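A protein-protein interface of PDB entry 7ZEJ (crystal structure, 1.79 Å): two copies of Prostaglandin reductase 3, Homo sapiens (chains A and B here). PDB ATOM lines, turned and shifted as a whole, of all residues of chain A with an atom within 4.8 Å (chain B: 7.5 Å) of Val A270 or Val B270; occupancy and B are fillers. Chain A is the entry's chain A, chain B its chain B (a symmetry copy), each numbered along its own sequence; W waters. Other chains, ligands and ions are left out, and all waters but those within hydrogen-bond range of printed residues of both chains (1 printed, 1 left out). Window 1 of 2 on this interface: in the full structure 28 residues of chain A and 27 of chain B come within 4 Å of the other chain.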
ATOM      1  N   PHE A 223      -1.925   5.507  27.879  1.00  0.00           N
ATOM      2  CA  PHE A 223      -0.790   6.038  27.080  1.00  0.00           C
ATOM      3  C   PHE A 223       0.420   6.334  27.993  1.00  0.00           C
ATOM      4  O   PHE A 223       1.528   5.831  27.709  1.00  0.00           O
ATOM      5  CB  PHE A 223      -1.225   7.269  26.283  1.00  0.00           C
ATOM      6  CG  PHE A 223      -0.130   7.962  25.522  1.00  0.00           C
ATOM      7  CD1 PHE A 223       0.261   7.515  24.269  1.00  0.00           C
ATOM      8  CD2 PHE A 223       0.509   9.074  26.048  1.00  0.00           C
ATOM      9  CE1 PHE A 223       1.250   8.160  23.547  1.00  0.00           C
ATOM     10  CE2 PHE A 223       1.525   9.699  25.341  1.00  0.00           C
ATOM     11  CZ  PHE A 223       1.897   9.243  24.092  1.00  0.00           C
ATOM     12  N   LEU A 236       5.962   2.857  20.353  1.00  0.00           N
ATOM     13  CA  LEU A 236       4.538   3.015  20.712  1.00  0.00           C
ATOM     14  C   LEU A 236       3.797   3.485  19.458  1.00  0.00           C
ATOM     15  O   LEU A 236       4.156   4.527  18.905  1.00  0.00           O
ATOM     16  CB  LEU A 236       4.358   3.969  21.893  1.00  0.00           C
ATOM     17  CG  LEU A 236       2.941   4.050  22.469  1.00  0.00           C
ATOM     18  CD1 LEU A 236       2.982   4.719  23.816  1.00  0.00           C
ATOM     19  CD2 LEU A 236       1.995   4.800  21.547  1.00  0.00           C
ATOM     20  N   VAL A 238       0.457   4.964  18.002  1.00  0.00           N
ATOM     21  CA  VAL A 238      -0.829   5.641  18.321  1.00  0.00           C
ATOM     22  C   VAL A 238      -1.837   5.260  17.242  1.00  0.00           C
ATOM     23  O   VAL A 238      -1.871   5.921  16.165  1.00  0.00           O
ATOM     24  CB  VAL A 238      -0.704   7.169  18.445  1.00  0.00           C
ATOM     25  CG1 VAL A 238      -2.013   7.776  18.923  1.00  0.00           C
ATOM     26  CG2 VAL A 238       0.425   7.565  19.375  1.00  0.00           C
ATOM     27  N   LEU A 259       7.721  13.602  27.826  1.00  0.00           N
ATOM     28  CA  LEU A 259       7.706  12.534  26.789  1.00  0.00           C
ATOM     29  C   LEU A 259       8.986  12.594  25.955  1.00  0.00           C
ATOM     30  O   LEU A 259       9.570  11.551  25.718  1.00  0.00           O
ATOM     31  CB  LEU A 259       6.454  12.655  25.911  1.00  0.00           C
ATOM     32  CG  LEU A 259       6.404  11.723  24.698  1.00  0.00           C
ATOM     33  CD1 LEU A 259       6.399  10.268  25.136  1.00  0.00           C
ATOM     34  CD2 LEU A 259       5.158  12.006  23.846  1.00  0.00           C
ATOM     35  N   LEU A 263      11.671   9.382  25.614  1.00  0.00           N
ATOM     36  CA  LEU A 263      11.971   8.789  24.281  1.00  0.00           C
ATOM     37  C   LEU A 263      13.475   8.912  24.003  1.00  0.00           C
ATOM     38  O   LEU A 263      14.081   7.922  23.535  1.00  0.00           O
ATOM     39  CB  LEU A 263      11.147   9.494  23.190  1.00  0.00           C
ATOM     40  CG  LEU A 263       9.625   9.351  23.291  1.00  0.00           C
ATOM     41  CD1 LEU A 263       8.942  10.041  22.126  1.00  0.00           C
ATOM     42  CD2 LEU A 263       9.205   7.887  23.368  1.00  0.00           C
ATOM     43  N   ALA A 268      13.504   5.490  22.090  1.00  0.00           N
ATOM     44  CA  ALA A 268      12.170   4.921  21.769  1.00  0.00           C
ATOM     45  C   ALA A 268      11.391   5.907  20.890  1.00  0.00           C
ATOM     46  O   ALA A 268      11.784   7.099  20.787  1.00  0.00           O
ATOM     47  CB  ALA A 268      11.426   4.581  23.048  1.00  0.00           C
ATOM     48  N   SER A 269      10.295   5.444  20.292  1.00  0.00           N
ATOM     49  CA  SER A 269       9.468   6.267  19.361  1.00  0.00           C
ATOM     50  C   SER A 269       7.974   6.193  19.686  1.00  0.00           C
ATOM     51  O   SER A 269       7.485   5.183  20.240  1.00  0.00           O
ATOM     52  CB  SER A 269       9.693   5.854  17.934  1.00  0.00           C
ATOM     53  OG  SER A 269       9.416   4.465  17.805  1.00  0.00           O
ATOM     54  N   VAL A 270       7.277   7.248  19.293  1.00  0.00           N
ATOM     55  CA  VAL A 270       5.801   7.340  19.288  1.00  0.00           C
ATOM     56  C   VAL A 270       5.443   7.596  17.847  1.00  0.00           C
ATOM     57  O   VAL A 270       5.905   8.618  17.286  1.00  0.00           O
ATOM     58  CB  VAL A 270       5.274   8.442  20.222  1.00  0.00           C
ATOM     59  CG1 VAL A 270       3.816   8.754  19.932  1.00  0.00           C
ATOM     60  CG2 VAL A 270       5.479   8.064  21.680  1.00  0.00           C
ATOM     61  N   GLN A 271       4.695   6.683  17.249  1.00  0.00           N
ATOM     62  CA  GLN A 271       4.436   6.725  15.795  1.00  0.00           C
ATOM     63  C   GLN A 271       2.920   6.720  15.613  1.00  0.00           C
ATOM     64  O   GLN A 271       2.281   5.732  16.014  1.00  0.00           O
ATOM     65  CB  GLN A 271       5.167   5.535  15.152  1.00  0.00           C
ATOM     66  CG  GLN A 271       4.668   5.155  13.763  1.00  0.00           C
ATOM     67  CD  GLN A 271       5.261   6.002  12.654  1.00  0.00           C
ATOM     68  OE1 GLN A 271       6.443   5.906  12.336  1.00  0.00           O
ATOM     69  NE2 GLN A 271       4.443   6.872  12.073  1.00  0.00           N
ATOM     70  N   GLY A 272       2.393   7.763  14.983  1.00  0.00           N
ATOM     71  CA  GLY A 272       0.989   7.837  14.570  1.00  0.00           C
ATOM     72  C   GLY A 272       0.680   6.923  13.388  1.00  0.00           C
ATOM     73  O   GLY A 272       1.556   6.667  12.531  1.00  0.00           O
ATOM     74  N   PHE B 223      10.868  22.746  19.074  1.00  0.00           N
ATOM     75  CA  PHE B 223      10.213  21.422  18.980  1.00  0.00           C
ATOM     76  C   PHE B 223       8.763  21.562  18.478  1.00  0.00           C
ATOM     77  O   PHE B 223       8.364  20.814  17.548  1.00  0.00           O
ATOM     78  CB  PHE B 223      10.279  20.703  20.320  1.00  0.00           C
ATOM     79  CG  PHE B 223       9.586  19.362  20.337  1.00  0.00           C
ATOM     80  CD1 PHE B 223      10.259  18.212  19.950  1.00  0.00           C
ATOM     81  CD2 PHE B 223       8.278  19.252  20.775  1.00  0.00           C
ATOM     82  CE1 PHE B 223       9.643  16.980  20.000  1.00  0.00           C
ATOM     83  CE2 PHE B 223       7.651  18.019  20.814  1.00  0.00           C
ATOM     84  CZ  PHE B 223       8.333  16.889  20.422  1.00  0.00           C
ATOM     85  N   VAL B 227       7.108  20.053  15.041  1.00  0.00           N
ATOM     86  CA  VAL B 227       5.938  19.127  15.037  1.00  0.00           C
ATOM     87  C   VAL B 227       4.898  19.652  14.037  1.00  0.00           C
ATOM     88  O   VAL B 227       4.443  18.880  13.179  1.00  0.00           O
ATOM     89  CB  VAL B 227       5.353  18.946  16.447  1.00  0.00           C
ATOM     90  CG1 VAL B 227       4.006  18.220  16.428  1.00  0.00           C
ATOM     91  CG2 VAL B 227       6.334  18.193  17.337  1.00  0.00           C
ATOM     92  N   LEU B 230       5.757  19.142  10.232  1.00  0.00           N
ATOM     93  CA  LEU B 230       5.943  17.775   9.676  1.00  0.00           C
ATOM     94  C   LEU B 230       4.971  17.542   8.507  1.00  0.00           C
ATOM     95  O   LEU B 230       3.808  17.922   8.622  1.00  0.00           O
ATOM     96  CB  LEU B 230       5.749  16.748  10.791  1.00  0.00           C
ATOM     97  CG  LEU B 230       6.913  16.630  11.781  1.00  0.00           C
ATOM     98  CD1 LEU B 230       6.557  15.682  12.905  1.00  0.00           C
ATOM     99  CD2 LEU B 230       8.177  16.145  11.069  1.00  0.00           C
ATOM    100  N   GLY B 234       6.054  12.287   8.170  1.00  0.00           N
ATOM    101  CA  GLY B 234       7.264  12.970   8.664  1.00  0.00           C
ATOM    102  C   GLY B 234       7.852  12.311   9.913  1.00  0.00           C
ATOM    103  O   GLY B 234       7.118  11.618  10.654  1.00  0.00           O
ATOM    104  N   ARG B 235       9.150  12.524  10.147  1.00  0.00           N
ATOM    105  CA  ARG B 235       9.932  11.957  11.279  1.00  0.00           C
ATOM    106  C   ARG B 235      10.701  13.079  11.984  1.00  0.00           C
ATOM    107  O   ARG B 235      11.591  13.688  11.330  1.00  0.00           O
ATOM    108  CB  ARG B 235      10.958  10.934  10.789  1.00  0.00           C
ATOM    109  CG  ARG B 235      10.344   9.714  10.129  1.00  0.00           C
ATOM    110  CD  ARG B 235      11.421   8.784   9.654  1.00  0.00           C
ATOM    111  NE  ARG B 235      10.794   7.713   8.906  1.00  0.00           N
ATOM    112  CZ  ARG B 235      11.438   6.683   8.394  1.00  0.00           C
ATOM    113  NH1 ARG B 235      12.739   6.571   8.565  1.00  0.00           N
ATOM    114  NH2 ARG B 235      10.774   5.751   7.735  1.00  0.00           N
ATOM    115  N   LEU B 236      10.341  13.370  13.238  1.00  0.00           N
ATOM    116  CA  LEU B 236      11.102  14.288  14.100  1.00  0.00           C
ATOM    117  C   LEU B 236      11.995  13.429  15.005  1.00  0.00           C
ATOM    118  O   LEU B 236      11.460  12.626  15.797  1.00  0.00           O
ATOM    119  CB  LEU B 236      10.123  15.152  14.896  1.00  0.00           C
ATOM    120  CG  LEU B 236      10.774  16.242  15.753  1.00  0.00           C
ATOM    121  CD1 LEU B 236       9.761  17.325  16.063  1.00  0.00           C
ATOM    122  CD2 LEU B 236      11.362  15.668  17.035  1.00  0.00           C
ATOM    123  N   ILE B 237      13.310  13.541  14.827  1.00  0.00           N
ATOM    124  CA  ILE B 237      14.317  12.833  15.665  1.00  0.00           C
ATOM    125  C   ILE B 237      14.690  13.758  16.820  1.00  0.00           C
ATOM    126  O   ILE B 237      15.155  14.927  16.548  1.00  0.00           O
ATOM    127  CB  ILE B 237      15.555  12.410  14.850  1.00  0.00           C
ATOM    128  CG1 ILE B 237      15.177  11.555  13.633  1.00  0.00           C
ATOM    129  CG2 ILE B 237      16.509  11.678  15.766  1.00  0.00           C
ATOM    130  CD1 ILE B 237      16.331  11.299  12.659  1.00  0.00           C
ATOM    131  N   VAL B 238      14.447  13.294  18.042  1.00  0.00           N
ATOM    132  CA  VAL B 238      14.820  14.053  19.269  1.00  0.00           C
ATOM    133  C   VAL B 238      16.278  13.716  19.560  1.00  0.00           C
ATOM    134  O   VAL B 238      16.539  12.637  20.080  1.00  0.00           O
ATOM    135  CB  VAL B 238      13.913  13.754  20.480  1.00  0.00           C
ATOM    136  CG1 VAL B 238      14.384  14.496  21.722  1.00  0.00           C
ATOM    137  CG2 VAL B 238      12.470  14.054  20.171  1.00  0.00           C
ATOM    138  N   LEU B 259       0.054  16.288  21.148  1.00  0.00           N
ATOM    139  CA  LEU B 259       1.087  15.679  20.278  1.00  0.00           C
ATOM    140  C   LEU B 259       0.589  14.343  19.711  1.00  0.00           C
ATOM    141  O   LEU B 259       0.670  14.134  18.509  1.00  0.00           O
ATOM    142  CB  LEU B 259       2.387  15.499  21.057  1.00  0.00           C
ATOM    143  CG  LEU B 259       3.534  14.850  20.279  1.00  0.00           C
ATOM    144  CD1 LEU B 259       3.846  15.613  19.015  1.00  0.00           C
ATOM    145  CD2 LEU B 259       4.765  14.767  21.147  1.00  0.00           C
ATOM    146  N   PRO B 260       0.102  13.378  20.523  1.00  0.00           N
ATOM    147  CA  PRO B 260      -0.351  12.096  19.961  1.00  0.00           C
ATOM    148  C   PRO B 260      -1.424  12.255  18.874  1.00  0.00           C
ATOM    149  O   PRO B 260      -1.396  11.506  17.916  1.00  0.00           O
ATOM    150  CB  PRO B 260      -0.898  11.319  21.167  1.00  0.00           C
ATOM    151  CG  PRO B 260      -0.151  11.945  22.349  1.00  0.00           C
ATOM    152  CD  PRO B 260       0.011  13.413  21.991  1.00  0.00           C
ATOM    153  N   LEU B 263       0.310  13.477  15.614  1.00  0.00           N
ATOM    154  CA  LEU B 263       1.105  12.395  14.980  1.00  0.00           C
ATOM    155  C   LEU B 263       0.151  11.393  14.322  1.00  0.00           C
ATOM    156  O   LEU B 263       0.485  10.872  13.241  1.00  0.00           O
ATOM    157  CB  LEU B 263       1.961  11.687  16.027  1.00  0.00           C
ATOM    158  CG  LEU B 263       3.008  12.544  16.735  1.00  0.00           C
ATOM    159  CD1 LEU B 263       3.772  11.687  17.738  1.00  0.00           C
ATOM    160  CD2 LEU B 263       3.966  13.177  15.746  1.00  0.00           C
ATOM    161  N   LEU B 264      -0.994  11.121  14.953  1.00  0.00           N
ATOM    162  CA  LEU B 264      -1.971  10.181  14.344  1.00  0.00           C
ATOM    163  C   LEU B 264      -2.483  10.813  13.041  1.00  0.00           C
ATOM    164  O   LEU B 264      -2.409  10.158  12.007  1.00  0.00           O
ATOM    165  CB  LEU B 264      -3.074   9.834  15.343  1.00  0.00           C
ATOM    166  CG  LEU B 264      -4.111   8.848  14.805  1.00  0.00           C
ATOM    167  CD1 LEU B 264      -4.818   8.136  15.936  1.00  0.00           C
ATOM    168  CD2 LEU B 264      -5.116   9.581  13.927  1.00  0.00           C
ATOM    169  N   ALA B 268       2.675  10.420  11.575  1.00  0.00           N
ATOM    170  CA  ALA B 268       4.053  10.918  11.773  1.00  0.00           C
ATOM    171  C   ALA B 268       4.617  10.393  13.093  1.00  0.00           C
ATOM    172  O   ALA B 268       3.848   9.863  13.895  1.00  0.00           O
ATOM    173  CB  ALA B 268       4.063  12.428  11.675  1.00  0.00           C
ATOM    174  N   SER B 269       5.939  10.534  13.296  1.00  0.00           N
ATOM    175  CA  SER B 269       6.667   9.968  14.451  1.00  0.00           C
ATOM    176  C   SER B 269       7.562  11.013  15.130  1.00  0.00           C
ATOM    177  O   SER B 269       8.022  11.980  14.455  1.00  0.00           O
ATOM    178  CB  SER B 269       7.478   8.748  14.067  1.00  0.00           C
ATOM    179  OG  SER B 269       8.312   9.000  12.956  1.00  0.00           O
ATOM    180  N   VAL B 270       7.759  10.804  16.431  1.00  0.00           N
ATOM    181  CA  VAL B 270       8.801  11.444  17.278  1.00  0.00           C
ATOM    182  C   VAL B 270       9.667  10.296  17.774  1.00  0.00           C
ATOM    183  O   VAL B 270       9.106   9.332  18.355  1.00  0.00           O
ATOM    184  CB  VAL B 270       8.190  12.271  18.418  1.00  0.00           C
ATOM    185  CG1 VAL B 270       9.245  12.739  19.399  1.00  0.00           C
ATOM    186  CG2 VAL B 270       7.434  13.456  17.855  1.00  0.00           C
ATOM    187  N   GLN B 271      10.943  10.324  17.404  1.00  0.00           N
ATOM    188  CA  GLN B 271      11.879   9.205  17.649  1.00  0.00           C
ATOM    189  C   GLN B 271      13.044   9.799  18.432  1.00  0.00           C
ATOM    190  O   GLN B 271      13.604  10.785  17.957  1.00  0.00           O
ATOM    191  CB  GLN B 271      12.265   8.571  16.306  1.00  0.00           C
ATOM    192  CG  GLN B 271      13.464   7.639  16.347  1.00  0.00           C
ATOM    193  CD  GLN B 271      13.150   6.231  16.819  1.00  0.00           C
ATOM    194  OE1 GLN B 271      12.610   5.412  16.076  1.00  0.00           O
ATOM    195  NE2 GLN B 271      13.500   5.926  18.068  1.00  0.00           N
ATOM    196  N   GLY B 272      13.319   9.250  19.613  1.00  0.00           N
ATOM    197  CA  GLY B 272      14.489   9.582  20.438  1.00  0.00           C
ATOM    198  C   GLY B 272      15.714   8.842  19.939  1.00  0.00           C
ATOM    199  O   GLY B 272      15.584   7.719  19.410  1.00  0.00           O
HETATM  200  O   HOH W   1       6.772   8.609  10.653  1.00  0.00           O
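The backbone carbonyl oxygen (O) of Ala A268 lies within hydrogen-bond range of the side-chain amide nitrogen (NE2) of Gln B271 (3.4 Å). N of Gly B272 lies within hydrogen-bond range of O of Ala A268. The backbone NH of Val A270 is in hydrogen-bond range of the backbone carbonyl oxygen of Val B270, 2.9 Å away. The backbone NH (N) of Gly A272 lies within hydrogen-bond range of the backbone carbonyl oxygen (O) of Ala B268 (2.8 Å).
O of Leu A236 is in hydrogen-bond range of N of Gln A271. N of Val A238 lies within hydrogen-bond range of O of Gln A271. The backbone NH (N) of Ala A268 is in hydrogen-bond range of the backbone carbonyl oxygen (O) of Leu A263 (2.9 Å). The backbone NH (N) of Leu B236 is in hydrogen-bond range of the backbone carbonyl oxygen (O) of Ser B269, at 3.0 Å. N of Val B238 is in hydrogen-bond range of O of Gln B271 (2.6 Å). The backbone carbonyl oxygen (O) of Leu B263 sits at hydrogen-bond distance from the backbone NH (N) of Ala B268.
Among the printed residues, pairs that only touch across the chains: Val A270 with Ser B269, Ser A269 with Val B270, Gly A272 with Leu B263, Gln A271 with Ser B269, Ser A269 with Gln B271, Leu A263 with Gly B272, Gln A271 with Ala B268, Val A270 with Leu B263, Val A238 with Leu B264, Gly A272 with Leu B264, Phe A223 with Pro B260, Leu A263 with Val B270, Leu A259 with Leu B259 and Val A238 with Pro B260.
Of the printed residues of chain B, Phe A223 touches Pro B260. Of the printed residues of chain B, Val A238 touches Pro B260 (3.9 Å) and Leu B264 (3.7 Å). Of the printed residues of chain B, Leu A263 touches Val B270 and Gly B272. Of the printed residues of chain B, Ala A268 touches Gln B271 (3.4 Å) and Gly B272 (2.9 Å). Val A270 touches just these residues of chain B: Leu B263, Ser B269 and Val B270. Of the printed residues of chain B, Gln A271 touches Ala B268 and Ser B269. Phe B223 touches none of the printed residues of chain A. Of chain A, only Leu A263, Ser A269 and Val A270 come within 4 Å of Val B270. The nearest printed residue of chain B that does not touch Ala A268 is Val B270 (4.3 Å).
Of the 17 printed residues of chain B, 9 touch a printed residue of chain A. Printed residues of chain A that touch a printed residue of chain B: Phe A223, Val A238, Leu A259, Leu A263, Ala A268, Ser A269, Val A270, Gln A271 and Gly A272. Hydrophobic or aromatic side chains of chain A within 4 Å of the printed part of chain B: Phe A223, Val A238, Leu A259, Leu A263 and Val A270.
Leu A259 touches its own counterpart, Leu B259. Ala A268 touches Gly B272, and with the chains exchanged Gly A272 touches Ala B268. Ser A269 touches Val B270, and with the chains exchanged Val A270 touches Ser B269. Val B270 touches its own counterpart, Val A270. Of the 18 pairs that touch across the chains among the printed residues, 14 have their exchanged pair printed and touching as well.
Water W1 lies within hydrogen-bond range of OG of Ser B269, O of Gly B234 and OE1 of Gln A271.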
